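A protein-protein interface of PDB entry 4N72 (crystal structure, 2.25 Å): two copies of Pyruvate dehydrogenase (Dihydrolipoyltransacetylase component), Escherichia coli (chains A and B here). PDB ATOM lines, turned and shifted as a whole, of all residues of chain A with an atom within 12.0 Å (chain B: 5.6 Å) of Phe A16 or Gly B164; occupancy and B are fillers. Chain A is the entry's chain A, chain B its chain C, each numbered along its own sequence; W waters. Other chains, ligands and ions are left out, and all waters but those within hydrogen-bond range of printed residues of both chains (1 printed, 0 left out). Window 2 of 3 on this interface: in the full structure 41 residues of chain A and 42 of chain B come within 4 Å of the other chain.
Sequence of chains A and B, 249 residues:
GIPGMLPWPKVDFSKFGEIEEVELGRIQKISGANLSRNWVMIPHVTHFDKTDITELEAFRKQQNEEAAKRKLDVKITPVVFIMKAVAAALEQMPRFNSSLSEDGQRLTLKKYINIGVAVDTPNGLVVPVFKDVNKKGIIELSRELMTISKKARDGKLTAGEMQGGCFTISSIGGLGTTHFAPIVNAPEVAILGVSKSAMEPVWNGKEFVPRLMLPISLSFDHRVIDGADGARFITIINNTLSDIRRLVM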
ATOM      1  N   PRO A   9     -18.614 -25.880 -35.656  1.00  0.00           N
ATOM      2  CA  PRO A   9     -18.553 -24.445 -35.943  1.00  0.00           C
ATOM      3  C   PRO A   9     -17.181 -23.841 -35.656  1.00  0.00           C
ATOM      4  O   PRO A   9     -16.598 -24.087 -34.599  1.00  0.00           O
ATOM      5  CB  PRO A   9     -19.593 -23.860 -34.985  1.00  0.00           C
ATOM      6  CG  PRO A   9     -20.569 -24.967 -34.778  1.00  0.00           C
ATOM      7  CD  PRO A   9     -19.753 -26.223 -34.786  1.00  0.00           C
ATOM      8  N   LYS A  10     -16.666 -23.076 -36.612  1.00  0.00           N
ATOM      9  CA  LYS A  10     -15.448 -22.302 -36.413  1.00  0.00           C
ATOM     10  C   LYS A  10     -15.840 -20.862 -36.131  1.00  0.00           C
ATOM     11  O   LYS A  10     -16.555 -20.243 -36.920  1.00  0.00           O
ATOM     12  CB  LYS A  10     -14.553 -22.360 -37.655  1.00  0.00           C
ATOM     13  CG  LYS A  10     -13.668 -23.594 -37.751  1.00  0.00           C
ATOM     14  CD  LYS A  10     -13.162 -23.788 -39.169  1.00  0.00           C
ATOM     15  CE  LYS A  10     -14.296 -24.201 -40.093  1.00  0.00           C
ATOM     16  NZ  LYS A  10     -14.883 -25.498 -39.659  1.00  0.00           N
ATOM     17  N   VAL A  11     -15.397 -20.335 -34.995  1.00  0.00           N
ATOM     18  CA  VAL A  11     -15.658 -18.939 -34.663  1.00  0.00           C
ATOM     19  C   VAL A  11     -14.384 -18.269 -34.164  1.00  0.00           C
ATOM     20  O   VAL A  11     -13.641 -18.843 -33.367  1.00  0.00           O
ATOM     21  CB  VAL A  11     -16.752 -18.783 -33.576  1.00  0.00           C
ATOM     22  CG1 VAL A  11     -17.333 -17.379 -33.610  1.00  0.00           C
ATOM     23  CG2 VAL A  11     -17.862 -19.809 -33.754  1.00  0.00           C
ATOM     24  N   ASP A  12     -14.123 -17.060 -34.647  1.00  0.00           N
ATOM     25  CA  ASP A  12     -13.042 -16.257 -34.099  1.00  0.00           C
ATOM     26  C   ASP A  12     -13.524 -15.668 -32.783  1.00  0.00           C
ATOM     27  O   ASP A  12     -14.128 -14.595 -32.754  1.00  0.00           O
ATOM     28  CB  ASP A  12     -12.650 -15.141 -35.060  1.00  0.00           C
ATOM     29  CG  ASP A  12     -11.302 -14.529 -34.725  1.00  0.00           C
ATOM     30  OD1 ASP A  12     -11.214 -13.753 -33.747  1.00  0.00           O
ATOM     31  OD2 ASP A  12     -10.328 -14.822 -35.449  1.00  0.00           O
ATOM     32  N   PHE A  13     -13.256 -16.384 -31.697  1.00  0.00           N
ATOM     33  CA  PHE A  13     -13.774 -16.030 -30.377  1.00  0.00           C
ATOM     34  C   PHE A  13     -13.255 -14.698 -29.842  1.00  0.00           C
ATOM     35  O   PHE A  13     -13.798 -14.158 -28.876  1.00  0.00           O
ATOM     36  CB  PHE A  13     -13.442 -17.135 -29.376  1.00  0.00           C
ATOM     37  CG  PHE A  13     -14.140 -18.433 -29.650  1.00  0.00           C
ATOM     38  CD1 PHE A  13     -15.479 -18.461 -30.005  1.00  0.00           C
ATOM     39  CD2 PHE A  13     -13.452 -19.630 -29.556  1.00  0.00           C
ATOM     40  CE1 PHE A  13     -16.118 -19.664 -30.254  1.00  0.00           C
ATOM     41  CE2 PHE A  13     -14.083 -20.831 -29.806  1.00  0.00           C
ATOM     42  CZ  PHE A  13     -15.419 -20.848 -30.157  1.00  0.00           C
ATOM     43  N   SER A  14     -12.208 -14.169 -30.464  1.00  0.00           N
ATOM     44  CA  SER A  14     -11.585 -12.940 -29.991  1.00  0.00           C
ATOM     45  C   SER A  14     -12.302 -11.686 -30.508  1.00  0.00           C
ATOM     46  O   SER A  14     -11.955 -10.568 -30.121  1.00  0.00           O
ATOM     47  CB  SER A  14     -10.102 -12.911 -30.370  1.00  0.00           C
ATOM     48  OG  SER A  14      -9.484 -11.703 -29.961  1.00  0.00           O
ATOM     49  N   LYS A  15     -13.315 -11.871 -31.357  1.00  0.00           N
ATOM     50  CA  LYS A  15     -14.160 -10.760 -31.798  1.00  0.00           C
ATOM     51  C   LYS A  15     -15.081 -10.352 -30.662  1.00  0.00           C
ATOM     52  O   LYS A  15     -15.885  -9.425 -30.787  1.00  0.00           O
ATOM     53  CB  LYS A  15     -15.007 -11.166 -33.006  1.00  0.00           C
ATOM     54  CG  LYS A  15     -14.473 -10.688 -34.347  1.00  0.00           C
ATOM     55  CD  LYS A  15     -13.777 -11.806 -35.091  1.00  0.00           C
ATOM     56  CE  LYS A  15     -13.245 -11.335 -36.438  1.00  0.00           C
ATOM     57  NZ  LYS A  15     -12.455 -12.388 -37.133  1.00  0.00           N
ATOM     58  N   PHE A  16     -14.950 -11.064 -29.551  1.00  0.00           N
ATOM     59  CA  PHE A  16     -15.878 -10.939 -28.447  1.00  0.00           C
ATOM     60  C   PHE A  16     -15.189 -10.551 -27.146  1.00  0.00           C
ATOM     61  O   PHE A  16     -15.820  -9.995 -26.250  1.00  0.00           O
ATOM     62  CB  PHE A  16     -16.658 -12.241 -28.287  1.00  0.00           C
ATOM     63  CG  PHE A  16     -17.473 -12.600 -29.493  1.00  0.00           C
ATOM     64  CD1 PHE A  16     -18.578 -11.847 -29.844  1.00  0.00           C
ATOM     65  CD2 PHE A  16     -17.129 -13.683 -30.280  1.00  0.00           C
ATOM     66  CE1 PHE A  16     -19.332 -12.167 -30.954  1.00  0.00           C
ATOM     67  CE2 PHE A  16     -17.880 -14.010 -31.392  1.00  0.00           C
ATOM     68  CZ  PHE A  16     -18.984 -13.250 -31.729  1.00  0.00           C
ATOM     69  N   GLY A  17     -13.892 -10.825 -27.057  1.00  0.00           N
ATOM     70  CA  GLY A  17     -13.128 -10.495 -25.869  1.00  0.00           C
ATOM     71  C   GLY A  17     -11.882 -11.343 -25.727  1.00  0.00           C
ATOM     72  O   GLY A  17     -11.485 -12.043 -26.659  1.00  0.00           O
ATOM     73  N   GLU A  18     -11.262 -11.279 -24.553  1.00  0.00           N
ATOM     74  CA  GLU A  18     -10.056 -12.050 -24.279  1.00  0.00           C
ATOM     75  C   GLU A  18     -10.344 -13.546 -24.243  1.00  0.00           C
ATOM     76  O   GLU A  18     -11.362 -13.980 -23.705  1.00  0.00           O
ATOM     77  CB  GLU A  18      -9.425 -11.613 -22.954  1.00  0.00           C
ATOM     78  CG  GLU A  18      -8.764 -10.246 -22.995  1.00  0.00           C
ATOM     79  CD  GLU A  18      -7.565 -10.208 -23.924  1.00  0.00           C
ATOM     80  OE1 GLU A  18      -6.910 -11.258 -24.099  1.00  0.00           O
ATOM     81  OE2 GLU A  18      -7.282  -9.129 -24.485  1.00  0.00           O
ATOM     82  N   ILE A  19      -9.445 -14.328 -24.829  1.00  0.00           N
ATOM     83  CA  ILE A  19      -9.541 -15.781 -24.770  1.00  0.00           C
ATOM     84  C   ILE A  19      -8.199 -16.393 -24.391  1.00  0.00           C
ATOM     85  O   ILE A  19      -7.160 -15.734 -24.457  1.00  0.00           O
ATOM     86  CB  ILE A  19     -10.003 -16.394 -26.111  1.00  0.00           C
ATOM     87  CG1 ILE A  19      -8.961 -16.148 -27.204  1.00  0.00           C
ATOM     88  CG2 ILE A  19     -11.366 -15.848 -26.517  1.00  0.00           C
ATOM     89  CD1 ILE A  19      -9.283 -16.831 -28.517  1.00  0.00           C
ATOM     90  N   GLU A  20      -8.234 -17.658 -23.990  1.00  0.00           N
ATOM     91  CA  GLU A  20      -7.028 -18.400 -23.660  1.00  0.00           C
ATOM     92  C   GLU A  20      -7.182 -19.843 -24.111  1.00  0.00           C
ATOM     93  O   GLU A  20      -7.993 -20.589 -23.562  1.00  0.00           O
ATOM     94  CB  GLU A  20      -6.761 -18.354 -22.156  1.00  0.00           C
ATOM     95  CG  GLU A  20      -5.661 -19.298 -21.695  1.00  0.00           C
ATOM     96  CD  GLU A  20      -5.593 -19.420 -20.185  1.00  0.00           C
ATOM     97  OE1 GLU A  20      -6.259 -18.621 -19.494  1.00  0.00           O
ATOM     98  OE2 GLU A  20      -4.879 -20.317 -19.691  1.00  0.00           O
ATOM     99  N   LYS B 110     -12.966 -18.774 -22.406  1.00  0.00           N
ATOM    100  CA  LYS B 110     -13.433 -17.418 -22.670  1.00  0.00           C
ATOM    101  C   LYS B 110     -13.445 -16.578 -21.396  1.00  0.00           C
ATOM    102  O   LYS B 110     -13.867 -17.044 -20.339  1.00  0.00           O
ATOM    103  CB  LYS B 110     -14.824 -17.458 -23.302  1.00  0.00           C
ATOM    104  CG  LYS B 110     -14.912 -18.398 -24.496  1.00  0.00           C
ATOM    105  CD  LYS B 110     -16.320 -18.474 -25.061  1.00  0.00           C
ATOM    106  CE  LYS B 110     -16.376 -19.435 -26.239  1.00  0.00           C
ATOM    107  NZ  LYS B 110     -17.734 -19.515 -26.843  1.00  0.00           N
ATOM    108  N   TYR B 112     -14.824 -13.388 -21.409  1.00  0.00           N
ATOM    109  CA  TYR B 112     -16.060 -12.617 -21.471  1.00  0.00           C
ATOM    110  C   TYR B 112     -17.258 -13.521 -21.206  1.00  0.00           C
ATOM    111  O   TYR B 112     -17.206 -14.722 -21.475  1.00  0.00           O
ATOM    112  CB  TYR B 112     -16.199 -11.954 -22.843  1.00  0.00           C
ATOM    113  CG  TYR B 112     -16.175 -12.935 -23.994  1.00  0.00           C
ATOM    114  CD1 TYR B 112     -14.974 -13.330 -24.570  1.00  0.00           C
ATOM    115  CD2 TYR B 112     -17.353 -13.469 -24.503  1.00  0.00           C
ATOM    116  CE1 TYR B 112     -14.947 -14.230 -25.621  1.00  0.00           C
ATOM    117  CE2 TYR B 112     -17.334 -14.369 -25.552  1.00  0.00           C
ATOM    118  CZ  TYR B 112     -16.130 -14.746 -26.105  1.00  0.00           C
ATOM    119  OH  TYR B 112     -16.109 -15.640 -27.153  1.00  0.00           O
ATOM    120  N   ASN B 114     -21.136 -14.016 -22.146  1.00  0.00           N
ATOM    121  CA  ASN B 114     -22.332 -13.735 -22.917  1.00  0.00           C
ATOM    122  C   ASN B 114     -23.305 -14.891 -22.828  1.00  0.00           C
ATOM    123  O   ASN B 114     -22.930 -16.051 -22.992  1.00  0.00           O
ATOM    124  CB  ASN B 114     -21.987 -13.465 -24.377  1.00  0.00           C
ATOM    125  CG  ASN B 114     -20.849 -12.479 -24.535  1.00  0.00           C
ATOM    126  OD1 ASN B 114     -20.394 -11.869 -23.566  1.00  0.00           O
ATOM    127  ND2 ASN B 114     -20.383 -12.314 -25.768  1.00  0.00           N
ATOM    128  N   VAL B 129     -28.388 -13.408 -27.887  1.00  0.00           N
ATOM    129  CA  VAL B 129     -27.277 -13.386 -26.941  1.00  0.00           C
ATOM    130  C   VAL B 129     -27.163 -12.031 -26.251  1.00  0.00           C
ATOM    131  O   VAL B 129     -27.131 -10.989 -26.907  1.00  0.00           O
ATOM    132  CB  VAL B 129     -25.936 -13.708 -27.650  1.00  0.00           C
ATOM    133  CG1 VAL B 129     -24.746 -13.263 -26.802  1.00  0.00           C
ATOM    134  CG2 VAL B 129     -25.844 -15.191 -27.967  1.00  0.00           C
ATOM    135  N   LYS B 131     -24.874  -9.587 -23.953  1.00  0.00           N
ATOM    136  CA  LYS B 131     -23.448  -9.311 -23.752  1.00  0.00           C
ATOM    137  C   LYS B 131     -23.107  -8.792 -22.364  1.00  0.00           C
ATOM    138  O   LYS B 131     -23.718  -7.837 -21.905  1.00  0.00           O
ATOM    139  CB  LYS B 131     -22.987  -8.259 -24.769  1.00  0.00           C
ATOM    140  CG  LYS B 131     -21.493  -7.897 -24.714  1.00  0.00           C
ATOM    141  CD  LYS B 131     -20.572  -9.128 -24.655  1.00  0.00           C
ATOM    142  CE  LYS B 131     -19.117  -8.698 -24.964  1.00  0.00           C
ATOM    143  NZ  LYS B 131     -18.321  -8.059 -23.798  1.00  0.00           N
ATOM    144  N   MET B 162     -27.510 -12.882 -32.817  1.00  0.00           N
ATOM    145  CA  MET B 162     -27.615 -14.298 -32.481  1.00  0.00           C
ATOM    146  C   MET B 162     -26.284 -15.048 -32.527  1.00  0.00           C
ATOM    147  O   MET B 162     -26.236 -16.208 -32.941  1.00  0.00           O
ATOM    148  CB  MET B 162     -28.658 -14.988 -33.366  1.00  0.00           C
ATOM    149  CG  MET B 162     -30.077 -14.588 -33.004  1.00  0.00           C
ATOM    150  SD  MET B 162     -31.368 -15.756 -33.487  1.00  0.00           S
ATOM    151  CE  MET B 162     -31.619 -15.347 -35.213  1.00  0.00           C
ATOM    152  N   GLN B 163     -25.211 -14.389 -32.102  1.00  0.00           N
ATOM    153  CA  GLN B 163     -23.936 -15.080 -31.913  1.00  0.00           C
ATOM    154  C   GLN B 163     -23.055 -14.457 -30.831  1.00  0.00           C
ATOM    155  O   GLN B 163     -23.310 -13.349 -30.356  1.00  0.00           O
ATOM    156  CB  GLN B 163     -23.172 -15.244 -33.234  1.00  0.00           C
ATOM    157  CG  GLN B 163     -23.171 -14.024 -34.128  1.00  0.00           C
ATOM    158  CD  GLN B 163     -23.525 -14.362 -35.564  1.00  0.00           C
ATOM    159  OE1 GLN B 163     -23.755 -15.522 -35.906  1.00  0.00           O
ATOM    160  NE2 GLN B 163     -23.580 -13.344 -36.411  1.00  0.00           N
ATOM    161  N   GLY B 164     -22.026 -15.196 -30.431  1.00  0.00           N
ATOM    162  CA  GLY B 164     -21.130 -14.753 -29.381  1.00  0.00           C
ATOM    163  C   GLY B 164     -21.474 -15.375 -28.043  1.00  0.00           C
ATOM    164  O   GLY B 164     -20.951 -14.967 -27.006  1.00  0.00           O
ATOM    165  N   GLY B 165     -22.351 -16.374 -28.073  1.00  0.00           N
ATOM    166  CA  GLY B 165     -22.849 -16.999 -26.862  1.00  0.00           C
ATOM    167  C   GLY B 165     -21.848 -17.910 -26.182  1.00  0.00           C
ATOM    168  O   GLY B 165     -21.086 -18.621 -26.839  1.00  0.00           O
ATOM    169  N   CYS B 166     -21.856 -17.886 -24.854  1.00  0.00           N
ATOM    170  CA  CYS B 166     -20.982 -18.734 -24.057  1.00  0.00           C
ATOM    171  C   CYS B 166     -21.797 -19.822 -23.375  1.00  0.00           C
ATOM    172  O   CYS B 166     -21.257 -20.833 -22.926  1.00  0.00           O
ATOM    173  CB  CYS B 166     -20.269 -17.904 -22.989  1.00  0.00           C
ATOM    174  SG  CYS B 166     -19.308 -16.512 -23.620  1.00  0.00           S
HETATM  175  O   HOH W   1     -18.780 -10.319 -27.345  1.00  0.00           O
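Lys A10 touches none of the printed residues of chain B. Phe A16 touches just these residues of chain B: Tyr B112, Lys B131 and Gly B164. Of the printed residues of chain B, Glu A18 touches Tyr B112 (3.8 Å). Printed residues of chain A within 4 Å of Lys B110: Phe A13 (3.8 Å). Tyr B112 touches just these residues of chain A: Phe A13, Phe A16, Gly A17 and Glu A18. No residue of chain A comes within 4 Å of Val B129. No residue of chain A comes within 4 Å of Gln B163. Gly B164 touches just one residue of chain A: Phe A16. The nearest residue of chain A that does not touch Gly B164 is Val A11 (6.1 Å).
Water W1 lies within hydrogen-bond range of the side-chain amide nitrogen (ND2) of Asn B114 and the backbone carbonyl oxygen (O) of Phe A16.
Among the printed residues, merely in contact across the chains: Phe A13 with Lys B110, Phe A16 with Tyr B112, Phe A16 with Lys B131, Phe A16 with Gly B164, Gly A17 with Tyr B112 and Glu A18 with Tyr B112.
The backbone carbonyl oxygen of Phe A13 sits at hydrogen-bond distance from the side-chain hydroxyl of Tyr B112 (3.2 Å).
NZ of Lys B110 lies within hydrogen-bond range of O of Gly B165 (3.5 Å). The backbone carbonyl oxygen (O) of Tyr B112 lies close to the side-chain sulfur (SG) of Cys B166. The backbone carbonyl oxygen (O) of Gly B164 is in hydrogen-bond range of the side-chain amide nitrogen (ND2) of Asn B114.
Hydrophobic or aromatic side chains of chain B that line the printed part of chain A: Tyr B112. Of the 12 printed residues of chain A, 4 touch a printed residue of chain B. Printed residues of chain A that touch a printed residue of chain B: Phe A13, Phe A16, Gly A17 and Glu A18. Hydrophobic or aromatic side chains of chain A that line the printed part of chain B: Phe A13 and Phe A16. Among the printed residues, no Asp or Glu carboxylate lies within 4 Å of a Lys or Arg side-chain nitrogen of the other chain.
No position is printed for both chains. Of the 7 pairs that touch across the chains among the printed residues, none has its exchanged pair printed and touching as well.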
